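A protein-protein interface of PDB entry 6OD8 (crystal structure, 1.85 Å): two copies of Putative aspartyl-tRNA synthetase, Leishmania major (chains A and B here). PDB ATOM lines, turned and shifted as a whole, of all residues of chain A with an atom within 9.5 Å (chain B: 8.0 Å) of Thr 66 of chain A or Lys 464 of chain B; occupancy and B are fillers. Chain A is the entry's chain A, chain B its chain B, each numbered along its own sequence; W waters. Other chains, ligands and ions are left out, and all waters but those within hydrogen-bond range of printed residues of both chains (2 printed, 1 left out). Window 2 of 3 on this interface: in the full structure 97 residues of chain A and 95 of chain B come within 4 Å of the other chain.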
ATOM      1  N   PRO A  61     -14.941 -20.425 -19.461  1.00  0.00           N
ATOM      2  CA  PRO A  61     -13.986 -21.177 -18.635  1.00  0.00           C
ATOM      3  C   PRO A  61     -14.684 -22.353 -17.966  1.00  0.00           C
ATOM      4  O   PRO A  61     -15.863 -22.279 -17.615  1.00  0.00           O
ATOM      5  CB  PRO A  61     -13.514 -20.147 -17.601  1.00  0.00           C
ATOM      6  CG  PRO A  61     -13.753 -18.827 -18.244  1.00  0.00           C
ATOM      7  CD  PRO A  61     -14.999 -19.005 -19.080  1.00  0.00           C
ATOM      8  N   MET A  62     -13.942 -23.446 -17.808  1.00  0.00           N
ATOM      9  CA  MET A  62     -14.495 -24.628 -17.153  1.00  0.00           C
ATOM     10  C   MET A  62     -14.956 -24.283 -15.742  1.00  0.00           C
ATOM     11  O   MET A  62     -14.283 -23.556 -15.008  1.00  0.00           O
ATOM     12  CB  MET A  62     -13.447 -25.739 -17.098  1.00  0.00           C
ATOM     13  CG  MET A  62     -13.985 -27.083 -16.584  1.00  0.00           C
ATOM     14  SD  MET A  62     -12.651 -28.277 -16.425  1.00  0.00           S
ATOM     15  CE  MET A  62     -11.473 -27.422 -15.375  1.00  0.00           C
ATOM     16  N   VAL A  63     -16.116 -24.807 -15.362  1.00  0.00           N
ATOM     17  CA  VAL A  63     -16.630 -24.591 -14.017  1.00  0.00           C
ATOM     18  C   VAL A  63     -15.717 -25.325 -13.045  1.00  0.00           C
ATOM     19  O   VAL A  63     -15.559 -26.547 -13.130  1.00  0.00           O
ATOM     20  CB  VAL A  63     -18.082 -25.074 -13.908  1.00  0.00           C
ATOM     21  CG1 VAL A  63     -18.567 -25.047 -12.459  1.00  0.00           C
ATOM     22  CG2 VAL A  63     -18.984 -24.235 -14.823  1.00  0.00           C
ATOM     23  N   GLN A  64     -15.093 -24.579 -12.122  1.00  0.00           N
ATOM     24  CA  GLN A  64     -14.058 -25.176 -11.281  1.00  0.00           C
ATOM     25  C   GLN A  64     -14.070 -24.604  -9.861  1.00  0.00           C
ATOM     26  O   GLN A  64     -13.019 -24.542  -9.217  1.00  0.00           O
ATOM     27  CB  GLN A  64     -12.677 -24.996 -11.940  1.00  0.00           C
ATOM     28  CG  GLN A  64     -11.604 -26.010 -11.516  1.00  0.00           C
ATOM     29  CD  GLN A  64     -10.271 -25.856 -12.247  1.00  0.00           C
ATOM     30  OE1 GLN A  64     -10.142 -25.084 -13.209  1.00  0.00           O
ATOM     31  NE2 GLN A  64      -9.277 -26.617 -11.810  1.00  0.00           N
ATOM     32  N   SER A  65     -15.243 -24.206  -9.346  1.00  0.00           N
ATOM     33  CA  SER A  65     -15.384 -23.767  -7.949  1.00  0.00           C
ATOM     34  C   SER A  65     -14.473 -22.575  -7.642  1.00  0.00           C
ATOM     35  O   SER A  65     -13.764 -22.541  -6.630  1.00  0.00           O
ATOM     36  CB  SER A  65     -15.116 -24.914  -6.974  1.00  0.00           C
ATOM     37  OG  SER A  65     -16.034 -25.961  -7.214  1.00  0.00           O
ATOM     38  N   THR A  66     -14.505 -21.588  -8.533  1.00  0.00           N
ATOM     39  CA  THR A  66     -13.806 -20.326  -8.308  1.00  0.00           C
ATOM     40  C   THR A  66     -14.743 -19.211  -7.858  1.00  0.00           C
ATOM     41  O   THR A  66     -14.263 -18.162  -7.412  1.00  0.00           O
ATOM     42  CB  THR A  66     -13.062 -19.903  -9.586  1.00  0.00           C
ATOM     43  OG1 THR A  66     -14.004 -19.675 -10.634  1.00  0.00           O
ATOM     44  CG2 THR A  66     -12.098 -20.986 -10.032  1.00  0.00           C
ATOM     45  N   THR A  67     -16.059 -19.391  -8.000  1.00  0.00           N
ATOM     46  CA  THR A  67     -17.050 -18.440  -7.521  1.00  0.00           C
ATOM     47  C   THR A  67     -18.137 -19.211  -6.788  1.00  0.00           C
ATOM     48  O   THR A  67     -18.366 -20.382  -7.063  1.00  0.00           O
ATOM     49  CB  THR A  67     -17.682 -17.640  -8.672  1.00  0.00           C
ATOM     50  OG1 THR A  67     -18.334 -18.545  -9.568  1.00  0.00           O
ATOM     51  CG2 THR A  67     -16.620 -16.838  -9.438  1.00  0.00           C
ATOM     52  N   TYR A  68     -18.831 -18.546  -5.871  1.00  0.00           N
ATOM     53  CA  TYR A  68     -19.932 -19.180  -5.148  1.00  0.00           C
ATOM     54  C   TYR A  68     -21.103 -18.210  -5.103  1.00  0.00           C
ATOM     55  O   TYR A  68     -20.949 -17.079  -4.630  1.00  0.00           O
ATOM     56  CB  TYR A  68     -19.478 -19.592  -3.742  1.00  0.00           C
ATOM     57  CG  TYR A  68     -20.544 -20.078  -2.775  1.00  0.00           C
ATOM     58  CD1 TYR A  68     -21.188 -21.306  -2.955  1.00  0.00           C
ATOM     59  CD2 TYR A  68     -20.872 -19.321  -1.653  1.00  0.00           C
ATOM     60  CE1 TYR A  68     -22.142 -21.743  -2.025  1.00  0.00           C
ATOM     61  CE2 TYR A  68     -21.811 -19.749  -0.734  1.00  0.00           C
ATOM     62  CZ  TYR A  68     -22.432 -20.960  -0.915  1.00  0.00           C
ATOM     63  OH  TYR A  68     -23.375 -21.335   0.023  1.00  0.00           O
ATOM     64  N   LYS A  69     -22.263 -18.651  -5.606  1.00  0.00           N
ATOM     65  CA  LYS A  69     -23.484 -17.837  -5.597  1.00  0.00           C
ATOM     66  C   LYS A  69     -23.245 -16.469  -6.242  1.00  0.00           C
ATOM     67  O   LYS A  69     -23.757 -15.439  -5.794  1.00  0.00           O
ATOM     68  CB  LYS A  69     -24.033 -17.687  -4.173  1.00  0.00           C
ATOM     69  CG  LYS A  69     -24.596 -19.011  -3.619  1.00  0.00           C
ATOM     70  CD  LYS A  69     -25.288 -18.836  -2.256  1.00  0.00           C
ATOM     71  CE  LYS A  69     -26.009 -20.159  -1.854  1.00  0.00           C
ATOM     72  NZ  LYS A  69     -26.787 -20.115  -0.567  1.00  0.00           N
ATOM     73  N   SER A  70     -22.447 -16.450  -7.300  1.00  0.00           N
ATOM     74  CA  SER A  70     -22.144 -15.166  -7.915  1.00  0.00           C
ATOM     75  C   SER A  70     -23.162 -14.770  -8.976  1.00  0.00           C
ATOM     76  O   SER A  70     -23.245 -13.586  -9.316  1.00  0.00           O
ATOM     77  CB  SER A  70     -20.738 -15.178  -8.518  1.00  0.00           C
ATOM     78  OG  SER A  70     -20.677 -16.065  -9.612  1.00  0.00           O
ATOM     79  N   GLU B 322     -21.826 -23.522  -9.809  1.00  0.00           N
ATOM     80  CA  GLU B 322     -20.529 -22.838  -9.712  1.00  0.00           C
ATOM     81  C   GLU B 322     -19.489 -23.553  -8.871  1.00  0.00           C
ATOM     82  O   GLU B 322     -18.303 -23.467  -9.202  1.00  0.00           O
ATOM     83  CB  GLU B 322     -20.699 -21.427  -9.126  1.00  0.00           C
ATOM     84  CG  GLU B 322     -21.573 -20.548  -9.992  1.00  0.00           C
ATOM     85  CD  GLU B 322     -21.834 -19.197  -9.377  1.00  0.00           C
ATOM     86  OE1 GLU B 322     -20.878 -18.583  -8.859  1.00  0.00           O
ATOM     87  OE2 GLU B 322     -23.000 -18.748  -9.438  1.00  0.00           O
ATOM     88  N   HIS B 323     -19.881 -24.209  -7.775  1.00  0.00           N
ATOM     89  CA  HIS B 323     -18.927 -24.497  -6.701  1.00  0.00           C
ATOM     90  C   HIS B 323     -19.339 -25.753  -5.940  1.00  0.00           C
ATOM     91  O   HIS B 323     -20.516 -25.927  -5.624  1.00  0.00           O
ATOM     92  CB  HIS B 323     -18.877 -23.299  -5.730  1.00  0.00           C
ATOM     93  CG  HIS B 323     -17.597 -23.154  -4.959  1.00  0.00           C
ATOM     94  ND1 HIS B 323     -17.218 -24.034  -3.969  1.00  0.00           N
ATOM     95  CD2 HIS B 323     -16.645 -22.189  -4.986  1.00  0.00           C
ATOM     96  CE1 HIS B 323     -16.066 -23.650  -3.453  1.00  0.00           C
ATOM     97  NE2 HIS B 323     -15.703 -22.517  -4.038  1.00  0.00           N
ATOM     98  N   TYR B 324     -18.361 -26.568  -5.538  1.00  0.00           N
ATOM     99  CA  TYR B 324     -18.693 -27.726  -4.707  1.00  0.00           C
ATOM    100  C   TYR B 324     -19.252 -27.338  -3.332  1.00  0.00           C
ATOM    101  O   TYR B 324     -19.839 -28.201  -2.660  1.00  0.00           O
ATOM    102  CB  TYR B 324     -17.464 -28.645  -4.525  1.00  0.00           C
ATOM    103  CG  TYR B 324     -16.375 -28.124  -3.594  1.00  0.00           C
ATOM    104  CD1 TYR B 324     -16.276 -28.582  -2.278  1.00  0.00           C
ATOM    105  CD2 TYR B 324     -15.444 -27.165  -4.029  1.00  0.00           C
ATOM    106  CE1 TYR B 324     -15.287 -28.126  -1.434  1.00  0.00           C
ATOM    107  CE2 TYR B 324     -14.441 -26.711  -3.201  1.00  0.00           C
ATOM    108  CZ  TYR B 324     -14.362 -27.185  -1.906  1.00  0.00           C
ATOM    109  OH  TYR B 324     -13.360 -26.702  -1.108  1.00  0.00           O
ATOM    110  N   ARG B 450     -10.812 -28.696   1.294  1.00  0.00           N
ATOM    111  CA  ARG B 450      -9.703 -28.591   0.346  1.00  0.00           C
ATOM    112  C   ARG B 450      -8.596 -29.604   0.606  1.00  0.00           C
ATOM    113  O   ARG B 450      -7.468 -29.221   0.954  1.00  0.00           O
ATOM    114  CB  ARG B 450      -9.080 -27.185   0.360  1.00  0.00           C
ATOM    115  CG  ARG B 450      -9.738 -26.202  -0.558  1.00  0.00           C
ATOM    116  CD  ARG B 450      -8.763 -25.091  -0.908  1.00  0.00           C
ATOM    117  NE  ARG B 450      -9.128 -24.447  -2.162  1.00  0.00           N
ATOM    118  CZ  ARG B 450      -8.270 -23.816  -2.954  1.00  0.00           C
ATOM    119  NH1 ARG B 450      -6.985 -23.750  -2.621  1.00  0.00           N
ATOM    120  NH2 ARG B 450      -8.699 -23.263  -4.081  1.00  0.00           N
ATOM    121  N   MET B 461     -11.989 -33.083  -8.958  1.00  0.00           N
ATOM    122  CA  MET B 461     -11.550 -31.832  -9.560  1.00  0.00           C
ATOM    123  C   MET B 461     -10.473 -31.166  -8.702  1.00  0.00           C
ATOM    124  O   MET B 461     -10.666 -30.940  -7.502  1.00  0.00           O
ATOM    125  CB  MET B 461     -12.756 -30.898  -9.737  1.00  0.00           C
ATOM    126  CG  MET B 461     -12.441 -29.599 -10.478  1.00  0.00           C
ATOM    127  SD  MET B 461     -12.122 -29.827 -12.240  1.00  0.00           S
ATOM    128  CE  MET B 461     -13.807 -29.808 -12.887  1.00  0.00           C
ATOM    129  N   GLU B 462      -9.335 -30.853  -9.320  1.00  0.00           N
ATOM    130  CA  GLU B 462      -8.272 -30.087  -8.668  1.00  0.00           C
ATOM    131  C   GLU B 462      -8.638 -28.600  -8.570  1.00  0.00           C
ATOM    132  O   GLU B 462      -9.458 -28.076  -9.335  1.00  0.00           O
ATOM    133  CB  GLU B 462      -6.954 -30.249  -9.434  1.00  0.00           C
ATOM    134  CG  GLU B 462      -6.342 -31.633  -9.277  1.00  0.00           C
ATOM    135  CD  GLU B 462      -5.464 -32.046 -10.448  1.00  0.00           C
ATOM    136  OE1 GLU B 462      -5.087 -31.168 -11.265  1.00  0.00           O
ATOM    137  OE2 GLU B 462      -5.156 -33.256 -10.546  1.00  0.00           O
ATOM    138  N   CYS B 463      -8.020 -27.919  -7.595  1.00  0.00           N
ATOM    139  CA  CYS B 463      -8.245 -26.486  -7.424  1.00  0.00           C
ATOM    140  C   CYS B 463      -7.562 -25.731  -8.549  1.00  0.00           C
ATOM    141  O   CYS B 463      -6.444 -26.074  -8.938  1.00  0.00           O
ATOM    142  CB  CYS B 463      -7.685 -25.998  -6.086  1.00  0.00           C
ATOM    143  SG  CYS B 463      -8.470 -26.761  -4.660  1.00  0.00           S
ATOM    144  N   LYS B 464      -8.235 -24.691  -9.066  1.00  0.00           N
ATOM    145  CA  LYS B 464      -7.674 -23.947 -10.198  1.00  0.00           C
ATOM    146  C   LYS B 464      -6.418 -23.183  -9.799  1.00  0.00           C
ATOM    147  O   LYS B 464      -5.484 -23.055 -10.598  1.00  0.00           O
ATOM    148  CB  LYS B 464      -8.710 -22.982 -10.769  1.00  0.00           C
ATOM    149  CG  LYS B 464      -8.183 -22.117 -11.919  1.00  0.00           C
ATOM    150  CD  LYS B 464      -9.330 -21.453 -12.653  1.00  0.00           C
ATOM    151  CE  LYS B 464      -8.825 -20.522 -13.740  1.00  0.00           C
ATOM    152  NZ  LYS B 464      -8.064 -19.380 -13.148  1.00  0.00           N
ATOM    153  N   ASP B 465      -6.366 -22.700  -8.566  1.00  0.00           N
ATOM    154  CA  ASP B 465      -5.256 -21.868  -8.119  1.00  0.00           C
ATOM    155  C   ASP B 465      -4.049 -22.681  -7.647  1.00  0.00           C
ATOM    156  O   ASP B 465      -2.941 -22.133  -7.564  1.00  0.00           O
ATOM    157  CB  ASP B 465      -5.754 -20.959  -6.995  1.00  0.00           C
ATOM    158  CG  ASP B 465      -6.487 -21.741  -5.907  1.00  0.00           C
ATOM    159  OD1 ASP B 465      -7.447 -22.485  -6.238  1.00  0.00           O
ATOM    160  OD2 ASP B 465      -6.084 -21.637  -4.727  1.00  0.00           O
ATOM    161  N   ASP B 466      -4.228 -23.976  -7.356  1.00  0.00           N
ATOM    162  CA  ASP B 466      -3.176 -24.763  -6.703  1.00  0.00           C
ATOM    163  C   ASP B 466      -3.536 -26.238  -6.878  1.00  0.00           C
ATOM    164  O   ASP B 466      -4.325 -26.768  -6.090  1.00  0.00           O
ATOM    165  CB  ASP B 466      -3.081 -24.377  -5.228  1.00  0.00           C
ATOM    166  CG  ASP B 466      -1.810 -24.889  -4.543  1.00  0.00           C
ATOM    167  OD1 ASP B 466      -1.235 -25.890  -5.006  1.00  0.00           O
ATOM    168  OD2 ASP B 466      -1.405 -24.290  -3.522  1.00  0.00           O
ATOM    169  N   VAL B 467      -2.965 -26.897  -7.892  1.00  0.00           N
ATOM    170  CA  VAL B 467      -3.415 -28.263  -8.177  1.00  0.00           C
ATOM    171  C   VAL B 467      -2.848 -29.254  -7.161  1.00  0.00           C
ATOM    172  O   VAL B 467      -3.106 -30.463  -7.253  1.00  0.00           O
ATOM    173  CB  VAL B 467      -3.077 -28.712  -9.617  1.00  0.00           C
ATOM    174  CG1 VAL B 467      -3.678 -27.764 -10.638  1.00  0.00           C
ATOM    175  CG2 VAL B 467      -1.593 -28.880  -9.813  1.00  0.00           C
ATOM    176  N   ARG B 468      -2.084 -28.757  -6.180  1.00  0.00           N
ATOM    177  CA  ARG B 468      -1.736 -29.593  -5.035  1.00  0.00           C
ATOM    178  C   ARG B 468      -2.957 -29.962  -4.197  1.00  0.00           C
ATOM    179  O   ARG B 468      -2.890 -30.902  -3.389  1.00  0.00           O
ATOM    180  CB  ARG B 468      -0.711 -28.880  -4.156  1.00  0.00           C
ATOM    181  CG  ARG B 468       0.643 -28.624  -4.839  1.00  0.00           C
ATOM    182  CD  ARG B 468       1.592 -27.850  -3.918  1.00  0.00           C
ATOM    183  NE  ARG B 468       0.939 -26.653  -3.393  1.00  0.00           N
ATOM    184  CZ  ARG B 468       1.353 -25.972  -2.332  1.00  0.00           C
ATOM    185  NH1 ARG B 468       2.434 -26.368  -1.675  1.00  0.00           N
ATOM    186  NH2 ARG B 468       0.680 -24.899  -1.919  1.00  0.00           N
ATOM    187  N   PHE B 469      -4.057 -29.235  -4.361  1.00  0.00           N
ATOM    188  CA  PHE B 469      -5.270 -29.417  -3.577  1.00  0.00           C
ATOM    189  C   PHE B 469      -6.455 -29.609  -4.510  1.00  0.00           C
ATOM    190  O   PHE B 469      -6.359 -29.411  -5.726  1.00  0.00           O
ATOM    191  CB  PHE B 469      -5.485 -28.218  -2.634  1.00  0.00           C
ATOM    192  CG  PHE B 469      -4.424 -28.102  -1.584  1.00  0.00           C
ATOM    193  CD1 PHE B 469      -4.514 -28.851  -0.414  1.00  0.00           C
ATOM    194  CD2 PHE B 469      -3.296 -27.292  -1.784  1.00  0.00           C
ATOM    195  CE1 PHE B 469      -3.508 -28.776   0.552  1.00  0.00           C
ATOM    196  CE2 PHE B 469      -2.288 -27.204  -0.818  1.00  0.00           C
ATOM    197  CZ  PHE B 469      -2.398 -27.947   0.350  1.00  0.00           C
ATOM    198  N   THR B 470      -7.589 -30.017  -3.933  1.00  0.00           N
ATOM    199  CA  THR B 470      -8.752 -30.406  -4.714  1.00  0.00           C
ATOM    200  C   THR B 470      -9.995 -29.748  -4.157  1.00  0.00           C
ATOM    201  O   THR B 470     -10.029 -29.285  -3.006  1.00  0.00           O
ATOM    202  CB  THR B 470      -8.971 -31.912  -4.702  1.00  0.00           C
ATOM    203  OG1 THR B 470      -9.064 -32.327  -3.341  1.00  0.00           O
ATOM    204  CG2 THR B 470      -7.831 -32.652  -5.403  1.00  0.00           C
ATOM    205  N   ASN B 471     -11.024 -29.731  -5.008  1.00  0.00           N
ATOM    206  CA  ASN B 471     -12.334 -29.170  -4.683  1.00  0.00           C
ATOM    207  C   ASN B 471     -13.141 -30.230  -3.937  1.00  0.00           C
ATOM    208  O   ASN B 471     -14.115 -30.797  -4.446  1.00  0.00           O
ATOM    209  CB  ASN B 471     -13.028 -28.706  -5.959  1.00  0.00           C
ATOM    210  CG  ASN B 471     -12.404 -27.444  -6.541  1.00  0.00           C
ATOM    211  OD1 ASN B 471     -11.739 -26.690  -5.839  1.00  0.00           O
ATOM    212  ND2 ASN B 471     -12.608 -27.216  -7.832  1.00  0.00           N
ATOM    213  N   GLN B 487     -16.435 -31.837  -5.937  1.00  0.00           N
ATOM    214  CA  GLN B 487     -16.714 -31.670  -7.358  1.00  0.00           C
ATOM    215  C   GLN B 487     -15.962 -32.733  -8.164  1.00  0.00           C
ATOM    216  O   GLN B 487     -14.787 -33.004  -7.904  1.00  0.00           O
ATOM    217  CB  GLN B 487     -16.279 -30.260  -7.832  1.00  0.00           C
ATOM    218  CG  GLN B 487     -16.478 -30.054  -9.334  1.00  0.00           C
ATOM    219  CD  GLN B 487     -16.042 -28.687  -9.837  1.00  0.00           C
ATOM    220  OE1 GLN B 487     -15.316 -27.946  -9.162  1.00  0.00           O
ATOM    221  NE2 GLN B 487     -16.475 -28.348 -11.040  1.00  0.00           N
HETATM  222  O   HOH W   1     -10.750 -24.056  -7.853  1.00  0.00           O
HETATM  223  O   HOH W   2     -12.218 -24.061  -4.780  1.00  0.00           O
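The backbone carbonyl oxygen (O) of Val 63 of chain A is in hydrogen-bond range of the side-chain amide nitrogen (NE2) of Gln 487 of chain B (2.9 Å). The side-chain amide nitrogen of Gln 64 of chain A sits at hydrogen-bond distance from the backbone carbonyl oxygen of Glu 462 of chain B (2.9 Å). The backbone carbonyl oxygen (O) of Gln 64 of chain A lies within hydrogen-bond range of the side-chain amide nitrogen (ND2) of Asn 471 of chain B (3.0 Å). N of Ser 65 of chain A is in hydrogen-bond range of O of Glu 322 of chain B (3.2 Å). O of Ser 65 of chain A is in hydrogen-bond range of NE2 of His 323 of chain B (3.2 Å). The side-chain hydroxyl of Ser 65 of chain A is in hydrogen-bond range of the backbone NH of Tyr 324 of chain B, at 2.9 Å. OE1 of Gln 487 of chain B lies within hydrogen-bond range of OG of Ser 65 of chain A (2.9 Å). The side-chain hydroxyl (OG1) of Thr 67 of chain A lies within hydrogen-bond range of the side-chain carboxylate (OE1) of Glu 322 of chain B (2.6 Å). OG of Ser 70 of chain A lies within hydrogen-bond range of OE1 of Glu 322 of chain B (2.6 Å).
NE of Arg 450 of chain B lies close to SG of Cys 463 of chain B (3.5 Å). The backbone NH (N) of Asn 471 of chain B sits at hydrogen-bond distance from the backbone carbonyl oxygen (O) of Met 461 of chain B, at 2.8 Å. O of Phe 469 of chain B is in hydrogen-bond range of N of Cys 463 of chain B (2.9 Å). The side-chain sulfur of Cys 463 of chain B sits close to the backbone carbonyl oxygen of Thr 470 of chain B. The side-chain amide oxygen (OD1) of Asn 471 of chain B sits at hydrogen-bond distance from the side-chain sulfur (SG) of Cys 463 of chain B (3.5 Å). O of Asn 471 of chain B sits at hydrogen-bond distance from N of Gln 487 of chain B (2.9 Å).
Among the printed residues, merely in contact across the chains: Val 63 of chain A with Glu 322 of chain B (3.6 Å), Val 63 of chain A with Met 461 of chain B (3.7 Å), Gln 64 of chain A with Met 461 of chain B (3.8 Å), Gln 64 of chain A with Cys 463 of chain B (3.8 Å), Gln 64 of chain A with Lys 464 of chain B (3.5 Å), Gln 64 of chain A with Gln 487 of chain B (3.6 Å), Ser 65 of chain A with Asn 471 of chain B (3.5 Å), Thr 66 of chain A with Lys 464 of chain B (3.8 Å), Thr 67 of chain A with His 323 of chain B (3.2 Å), Tyr 68 of chain A with Glu 322 of chain B (3.6 Å) and Lys 69 of chain A with Glu 322 of chain B (3.5 Å).
Of the printed residues of chain B, Val 63 of chain A touches Glu 322, Met 461 and Gln 487. Of chain B, only Lys 464 comes within 4 Å of Thr 66 of chain A. Of the printed residues of chain A, His 323 of chain B touches Ser 65 (3.2 Å) and Thr 67 (3.2 Å). Of chain A, only Gln 64 (3.8 Å) comes within 4 Å of Cys 463 of chain B. Lys 464 of chain B touches just these residues of chain A: Gln 64 and Thr 66. Asp 465 of chain B touches none of the printed residues of chain A. The nearest residue of chain B that does not touch Thr 66 of chain A is His 323 of chain B (4.2 Å). The nearest residue of chain A that does not touch Lys 464 of chain B is Met 62 of chain A (5.9 Å).
Hydrophobic or aromatic side chains of chain B within 4 Å of the printed part of chain A: His 323, Tyr 324 and Met 461. Of the 10 printed residues of chain A, 8 touch a printed residue of chain B. Among the printed residues, 20 pairs touch across the chains. Among the printed residues, no Asp or Glu carboxylate lies within 4 Å of a Lys or Arg side-chain nitrogen of the other chain.
No position is printed for both chains. Of the 20 pairs that touch across the chains among the printed residues, none has its exchanged pair printed and touching as well.
Water W1 lies within hydrogen-bond range of the backbone carbonyl oxygen of Gln 64 of chain A (2.7 Å), the backbone NH of Lys 464 of chain B (2.9 Å) and the side-chain amide oxygen of Asn 471 of chain B (3.5 Å). Water W2 lies within hydrogen-bond range of O of Ser 65 of chain A (2.9 Å) and OD1 of Asn 471 of chain B (2.9 Å).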
